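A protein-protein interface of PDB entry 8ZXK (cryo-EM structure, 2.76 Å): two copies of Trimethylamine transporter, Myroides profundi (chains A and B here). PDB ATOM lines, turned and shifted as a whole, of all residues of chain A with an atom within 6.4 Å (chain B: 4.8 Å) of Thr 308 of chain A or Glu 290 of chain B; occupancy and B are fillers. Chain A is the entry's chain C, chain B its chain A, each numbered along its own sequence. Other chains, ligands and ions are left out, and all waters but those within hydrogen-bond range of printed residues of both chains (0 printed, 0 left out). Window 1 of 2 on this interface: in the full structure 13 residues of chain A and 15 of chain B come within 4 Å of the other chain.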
ATOM      1  N   ILE A 300      23.080  23.105  18.677  1.00  0.00           N
ATOM      2  CA  ILE A 300      23.278  24.124  19.701  1.00  0.00           C
ATOM      3  C   ILE A 300      24.174  23.605  20.816  1.00  0.00           C
ATOM      4  O   ILE A 300      24.920  24.376  21.433  1.00  0.00           O
ATOM      5  CB  ILE A 300      21.920  24.604  20.243  1.00  0.00           C
ATOM      6  CG1 ILE A 300      20.938  24.828  19.093  1.00  0.00           C
ATOM      7  CG2 ILE A 300      22.085  25.880  21.048  1.00  0.00           C
ATOM      8  CD1 ILE A 300      19.573  25.293  19.538  1.00  0.00           C
ATOM      9  N   ASP A 301      24.113  22.304  21.104  1.00  0.00           N
ATOM     10  CA  ASP A 301      24.942  21.736  22.160  1.00  0.00           C
ATOM     11  C   ASP A 301      26.424  21.835  21.814  1.00  0.00           C
ATOM     12  O   ASP A 301      27.232  22.264  22.645  1.00  0.00           O
ATOM     13  CB  ASP A 301      24.535  20.282  22.406  1.00  0.00           C
ATOM     14  CG  ASP A 301      25.487  19.543  23.334  1.00  0.00           C
ATOM     15  OD1 ASP A 301      26.153  20.190  24.169  1.00  0.00           O
ATOM     16  OD2 ASP A 301      25.568  18.301  23.226  1.00  0.00           O
ATOM     17  N   THR A 304      27.845  25.839  21.018  1.00  0.00           N
ATOM     18  CA  THR A 304      28.063  26.690  22.178  1.00  0.00           C
ATOM     19  C   THR A 304      28.951  26.047  23.234  1.00  0.00           C
ATOM     20  O   THR A 304      29.258  26.697  24.237  1.00  0.00           O
ATOM     21  CB  THR A 304      26.722  27.065  22.809  1.00  0.00           C
ATOM     22  OG1 THR A 304      26.113  25.890  23.353  1.00  0.00           O
ATOM     23  CG2 THR A 304      25.797  27.672  21.770  1.00  0.00           C
ATOM     24  N   TRP A 305      29.359  24.796  23.040  1.00  0.00           N
ATOM     25  CA  TRP A 305      30.173  24.104  24.031  1.00  0.00           C
ATOM     26  C   TRP A 305      31.501  24.821  24.226  1.00  0.00           C
ATOM     27  O   TRP A 305      32.169  25.197  23.259  1.00  0.00           O
ATOM     28  CB  TRP A 305      30.404  22.658  23.599  1.00  0.00           C
ATOM     29  CG  TRP A 305      31.156  21.842  24.597  1.00  0.00           C
ATOM     30  CD1 TRP A 305      30.752  21.509  25.854  1.00  0.00           C
ATOM     31  CD2 TRP A 305      32.444  21.243  24.417  1.00  0.00           C
ATOM     32  NE1 TRP A 305      31.710  20.746  26.472  1.00  0.00           N
ATOM     33  CE2 TRP A 305      32.759  20.567  25.611  1.00  0.00           C
ATOM     34  CE3 TRP A 305      33.362  21.216  23.364  1.00  0.00           C
ATOM     35  CZ2 TRP A 305      33.952  19.872  25.779  1.00  0.00           C
ATOM     36  CZ3 TRP A 305      34.544  20.526  23.535  1.00  0.00           C
ATOM     37  CH2 TRP A 305      34.829  19.863  24.732  1.00  0.00           C
ATOM     38  N   ASN A 306      31.889  25.004  25.491  1.00  0.00           N
ATOM     39  CA  ASN A 306      33.090  25.756  25.828  1.00  0.00           C
ATOM     40  C   ASN A 306      34.056  24.975  26.710  1.00  0.00           C
ATOM     41  O   ASN A 306      35.073  25.539  27.132  1.00  0.00           O
ATOM     42  CB  ASN A 306      32.720  27.074  26.516  1.00  0.00           C
ATOM     43  CG  ASN A 306      32.818  28.262  25.587  1.00  0.00           C
ATOM     44  OD1 ASN A 306      33.890  28.580  25.079  1.00  0.00           O
ATOM     45  ND2 ASN A 306      31.694  28.929  25.361  1.00  0.00           N
ATOM     46  N   ASP A 307      33.774  23.702  26.994  1.00  0.00           N
ATOM     47  CA  ASP A 307      34.613  22.888  27.877  1.00  0.00           C
ATOM     48  C   ASP A 307      34.821  23.585  29.218  1.00  0.00           C
ATOM     49  O   ASP A 307      35.928  23.629  29.759  1.00  0.00           O
ATOM     50  CB  ASP A 307      35.952  22.561  27.213  1.00  0.00           C
ATOM     51  CG  ASP A 307      36.568  21.284  27.739  1.00  0.00           C
ATOM     52  OD1 ASP A 307      35.912  20.594  28.545  1.00  0.00           O
ATOM     53  OD2 ASP A 307      37.708  20.968  27.344  1.00  0.00           O
ATOM     54  N   THR A 308      33.736  24.142  29.756  1.00  0.00           N
ATOM     55  CA  THR A 308      33.833  24.985  30.943  1.00  0.00           C
ATOM     56  C   THR A 308      34.209  24.180  32.179  1.00  0.00           C
ATOM     57  O   THR A 308      35.102  24.572  32.940  1.00  0.00           O
ATOM     58  CB  THR A 308      32.509  25.714  31.170  1.00  0.00           C
ATOM     59  OG1 THR A 308      32.089  26.336  29.951  1.00  0.00           O
ATOM     60  CG2 THR A 308      32.664  26.770  32.245  1.00  0.00           C
ATOM     61  N   TYR A 309      33.538  23.052  32.398  1.00  0.00           N
ATOM     62  CA  TYR A 309      33.663  22.332  33.659  1.00  0.00           C
ATOM     63  C   TYR A 309      34.857  21.387  33.687  1.00  0.00           C
ATOM     64  O   TYR A 309      35.530  21.279  34.716  1.00  0.00           O
ATOM     65  CB  TYR A 309      32.371  21.567  33.944  1.00  0.00           C
ATOM     66  CG  TYR A 309      31.173  22.470  34.128  1.00  0.00           C
ATOM     67  CD1 TYR A 309      30.903  23.055  35.356  1.00  0.00           C
ATOM     68  CD2 TYR A 309      30.320  22.749  33.069  1.00  0.00           C
ATOM     69  CE1 TYR A 309      29.815  23.884  35.528  1.00  0.00           C
ATOM     70  CE2 TYR A 309      29.230  23.578  33.231  1.00  0.00           C
ATOM     71  CZ  TYR A 309      28.981  24.141  34.462  1.00  0.00           C
ATOM     72  OH  TYR A 309      27.896  24.968  34.631  1.00  0.00           O
ATOM     73  N   LEU A 310      35.134  20.690  32.584  1.00  0.00           N
ATOM     74  CA  LEU A 310      36.322  19.843  32.540  1.00  0.00           C
ATOM     75  C   LEU A 310      37.592  20.676  32.440  1.00  0.00           C
ATOM     76  O   LEU A 310      38.572  20.410  33.145  1.00  0.00           O
ATOM     77  CB  LEU A 310      36.232  18.859  31.375  1.00  0.00           C
ATOM     78  CG  LEU A 310      35.970  17.396  31.743  1.00  0.00           C
ATOM     79  CD1 LEU A 310      34.538  17.196  32.216  1.00  0.00           C
ATOM     80  CD2 LEU A 310      36.283  16.482  30.569  1.00  0.00           C
ATOM     81  N   GLY A 311      37.593  21.690  31.580  1.00  0.00           N
ATOM     82  CA  GLY A 311      38.778  22.513  31.395  1.00  0.00           C
ATOM     83  C   GLY A 311      39.969  21.751  30.859  1.00  0.00           C
ATOM     84  O   GLY A 311      41.096  21.954  31.327  1.00  0.00           O
ATOM     85  N   VAL B 136      26.169  20.635  35.409  1.00  0.00           N
ATOM     86  CA  VAL B 136      25.526  21.029  34.158  1.00  0.00           C
ATOM     87  C   VAL B 136      24.011  20.930  34.283  1.00  0.00           C
ATOM     88  O   VAL B 136      23.277  21.827  33.852  1.00  0.00           O
ATOM     89  CB  VAL B 136      26.055  20.177  32.990  1.00  0.00           C
ATOM     90  CG1 VAL B 136      25.241  20.432  31.734  1.00  0.00           C
ATOM     91  CG2 VAL B 136      27.520  20.476  32.739  1.00  0.00           C
ATOM     92  N   PHE B 283      35.712  31.678  33.787  1.00  0.00           N
ATOM     93  CA  PHE B 283      34.787  30.577  34.018  1.00  0.00           C
ATOM     94  C   PHE B 283      33.346  31.044  33.902  1.00  0.00           C
ATOM     95  O   PHE B 283      32.511  30.344  33.327  1.00  0.00           O
ATOM     96  CB  PHE B 283      35.033  29.943  35.387  1.00  0.00           C
ATOM     97  CG  PHE B 283      34.153  28.754  35.668  1.00  0.00           C
ATOM     98  CD1 PHE B 283      32.899  28.917  36.236  1.00  0.00           C
ATOM     99  CD2 PHE B 283      34.580  27.474  35.363  1.00  0.00           C
ATOM    100  CE1 PHE B 283      32.089  27.829  36.486  1.00  0.00           C
ATOM    101  CE2 PHE B 283      33.774  26.381  35.616  1.00  0.00           C
ATOM    102  CZ  PHE B 283      32.529  26.560  36.179  1.00  0.00           C
ATOM    103  N   LYS B 286      32.552  31.621  30.063  1.00  0.00           N
ATOM    104  CA  LYS B 286      32.436  30.356  29.349  1.00  0.00           C
ATOM    105  C   LYS B 286      31.203  29.585  29.797  1.00  0.00           C
ATOM    106  O   LYS B 286      30.487  29.012  28.969  1.00  0.00           O
ATOM    107  CB  LYS B 286      33.694  29.515  29.562  1.00  0.00           C
ATOM    108  CG  LYS B 286      34.961  30.137  29.011  1.00  0.00           C
ATOM    109  CD  LYS B 286      35.955  29.069  28.596  1.00  0.00           C
ATOM    110  CE  LYS B 286      36.295  28.154  29.755  1.00  0.00           C
ATOM    111  NZ  LYS B 286      37.220  27.065  29.345  1.00  0.00           N
ATOM    112  N   GLY B 287      30.943  29.560  31.105  1.00  0.00           N
ATOM    113  CA  GLY B 287      29.771  28.874  31.607  1.00  0.00           C
ATOM    114  C   GLY B 287      28.481  29.531  31.170  1.00  0.00           C
ATOM    115  O   GLY B 287      27.503  28.848  30.890  1.00  0.00           O
ATOM    116  N   TYR B 288      28.457  30.861  31.101  1.00  0.00           N
ATOM    117  CA  TYR B 288      27.271  31.549  30.609  1.00  0.00           C
ATOM    118  C   TYR B 288      26.963  31.128  29.182  1.00  0.00           C
ATOM    119  O   TYR B 288      25.837  30.714  28.873  1.00  0.00           O
ATOM    120  CB  TYR B 288      27.469  33.062  30.698  1.00  0.00           C
ATOM    121  CG  TYR B 288      26.279  33.871  30.234  1.00  0.00           C
ATOM    122  CD1 TYR B 288      24.996  33.564  30.662  1.00  0.00           C
ATOM    123  CD2 TYR B 288      26.439  34.943  29.368  1.00  0.00           C
ATOM    124  CE1 TYR B 288      23.908  34.299  30.241  1.00  0.00           C
ATOM    125  CE2 TYR B 288      25.357  35.684  28.942  1.00  0.00           C
ATOM    126  CZ  TYR B 288      24.094  35.358  29.382  1.00  0.00           C
ATOM    127  OH  TYR B 288      23.013  36.095  28.960  1.00  0.00           O
ATOM    128  N   VAL B 289      27.971  31.180  28.308  1.00  0.00           N
ATOM    129  CA  VAL B 289      27.748  30.815  26.908  1.00  0.00           C
ATOM    130  C   VAL B 289      27.323  29.354  26.796  1.00  0.00           C
ATOM    131  O   VAL B 289      26.308  29.028  26.165  1.00  0.00           O
ATOM    132  CB  VAL B 289      29.008  31.104  26.071  1.00  0.00           C
ATOM    133  CG1 VAL B 289      28.824  30.607  24.648  1.00  0.00           C
ATOM    134  CG2 VAL B 289      29.319  32.586  26.084  1.00  0.00           C
ATOM    135  N   GLU B 290      28.076  28.454  27.436  1.00  0.00           N
ATOM    136  CA  GLU B 290      27.801  27.027  27.313  1.00  0.00           C
ATOM    137  C   GLU B 290      26.468  26.651  27.945  1.00  0.00           C
ATOM    138  O   GLU B 290      25.729  25.826  27.398  1.00  0.00           O
ATOM    139  CB  GLU B 290      28.940  26.222  27.939  1.00  0.00           C
ATOM    140  CG  GLU B 290      28.642  24.746  28.103  1.00  0.00           C
ATOM    141  CD  GLU B 290      29.822  23.968  28.642  1.00  0.00           C
ATOM    142  OE1 GLU B 290      30.970  24.339  28.331  1.00  0.00           O
ATOM    143  OE2 GLU B 290      29.601  22.983  29.377  1.00  0.00           O
ATOM    144  N   ASN B 291      26.138  27.241  29.095  1.00  0.00           N
ATOM    145  CA  ASN B 291      24.908  26.905  29.796  1.00  0.00           C
ATOM    146  C   ASN B 291      23.690  27.433  29.060  1.00  0.00           C
ATOM    147  O   ASN B 291      22.665  26.753  28.995  1.00  0.00           O
ATOM    148  CB  ASN B 291      24.952  27.454  31.222  1.00  0.00           C
ATOM    149  CG  ASN B 291      25.844  26.640  32.133  1.00  0.00           C
ATOM    150  OD1 ASN B 291      26.029  25.441  31.933  1.00  0.00           O
ATOM    151  ND2 ASN B 291      26.407  27.290  33.142  1.00  0.00           N
ATOM    152  N   THR B 292      23.773  28.642  28.497  1.00  0.00           N
ATOM    153  CA  THR B 292      22.672  29.125  27.675  1.00  0.00           C
ATOM    154  C   THR B 292      22.496  28.253  26.438  1.00  0.00           C
ATOM    155  O   THR B 292      21.365  27.920  26.058  1.00  0.00           O
ATOM    156  CB  THR B 292      22.903  30.583  27.283  1.00  0.00           C
ATOM    157  OG1 THR B 292      23.534  31.273  28.367  1.00  0.00           O
ATOM    158  CG2 THR B 292      21.582  31.261  26.965  1.00  0.00           C
ATOM    159  N   GLY B 293      23.603  27.847  25.812  1.00  0.00           N
ATOM    160  CA  GLY B 293      23.500  26.970  24.659  1.00  0.00           C
ATOM    161  C   GLY B 293      22.895  25.620  24.992  1.00  0.00           C
ATOM    162  O   GLY B 293      22.103  25.080  24.222  1.00  0.00           O
ATOM    163  N   ALA B 294      23.265  25.054  26.143  1.00  0.00           N
ATOM    164  CA  ALA B 294      22.717  23.764  26.550  1.00  0.00           C
ATOM    165  C   ALA B 294      21.264  23.881  26.990  1.00  0.00           C
ATOM    166  O   ALA B 294      20.474  22.957  26.771  1.00  0.00           O
ATOM    167  CB  ALA B 294      23.564  23.167  27.672  1.00  0.00           C
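N of Asp 307 of chain A is in hydrogen-bond range of OE1 of Glu 290 of chain B (3.2 Å). OH of Tyr 309 of chain A is in hydrogen-bond range of ND2 of Asn 291 of chain B, 3.1 Å away. The backbone NH (N) of Asn 306 of chain A is in hydrogen-bond range of the side-chain carboxylate (OE1) of Glu 290 of chain B. O of Asn 306 of chain A is in hydrogen-bond range of NZ of Lys 286 of chain B (3.4 Å). The backbone carbonyl oxygen (O) of Lys 286 of chain B lies within hydrogen-bond range of the side-chain hydroxyl (OG1) of Thr 308 of chain A (3.3 Å). OE1 of Glu 290 of chain B is in hydrogen-bond range of OG1 of Thr 308 of chain A (2.8 Å).
The backbone carbonyl oxygen (O) of Thr 304 of chain A is in hydrogen-bond range of the side-chain amide nitrogen (ND2) of Asn 306 of chain A (3.5 Å). The backbone carbonyl oxygen (O) of Ile 300 of chain A is in hydrogen-bond range of the side-chain hydroxyl (OG1) of Thr 304 of chain A (2.7 Å). The side-chain amide nitrogen (ND2) of Asn 291 of chain B lies close to the backbone carbonyl oxygen (O) of Gly 287 of chain B.
CG2 of Ile 300 of chain A touches O of Gly 293 of chain B (3.3 Å). CB of Thr 304 of chain A touches O of Val 289 of chain B (3.9 Å). Thr 304 of chain A touches Gly 293 of chain B. Glu 290 of chain B touches Trp 305 of chain A (OE1 to CD1, 3.8 Å). Val 289 of chain B touches Asn 306 of chain A (CG1 to ND2, 3.4 Å). Lys 286 of chain B touches Asp 307 of chain A. Gly 287 of chain B touches Thr 308 of chain A. Tyr 309 of chain A touches Val 136 of chain B. CE1 of Tyr 309 of chain A touches CZ of Phe 283 of chain B, at 3.9 Å. Glu 290 of chain B touches Tyr 309 of chain A.
No position is printed for both chains.
Of the 10 printed residues of chain A, 7 touch a printed residue of chain B. Printed residues of chain A that touch a printed residue of chain B: Ile 300, Thr 304, Trp 305, Asn 306, Asp 307, Thr 308 and Tyr 309. Hydrophobic or aromatic side chains of chain A within 4 Å of the printed part of chain B: Ile 300, Trp 305 and Tyr 309. Of the 11 printed residues of chain B, 8 touch a printed residue of chain A. Hydrophobic or aromatic side chains of chain B that line the printed part of chain A: Val 136, Phe 283 and Val 289. Along chain B the printed residues that touch a printed residue of chain A span positions 136 to 293.
Of chain A, only Thr 304, Trp 305, Asn 306, Asp 307, Thr 308 and Tyr 309 come within 4 Å of Glu 290 of chain B. Of the printed residues of chain A, Val 289 of chain B touches Thr 304 and Asn 306. Of the printed residues of chain B, Trp 305 of chain A touches Glu 290. Printed residues of chain B within 4 Å of Thr 304 of chain A: Val 289, Glu 290 and Gly 293. Of the printed residues of chain A, Asn 291 of chain B touches Tyr 309 (3.1 Å). Tyr 288 of chain B touches none of the printed residues of chain A. The nearest printed residue of chain B that does not touch Thr 308 of chain A is Tyr 288 of chain B (5.9 Å). The nearest printed residue of chain B that does not touch Asn 306 of chain A is Gly 287 of chain B (5.5 Å).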
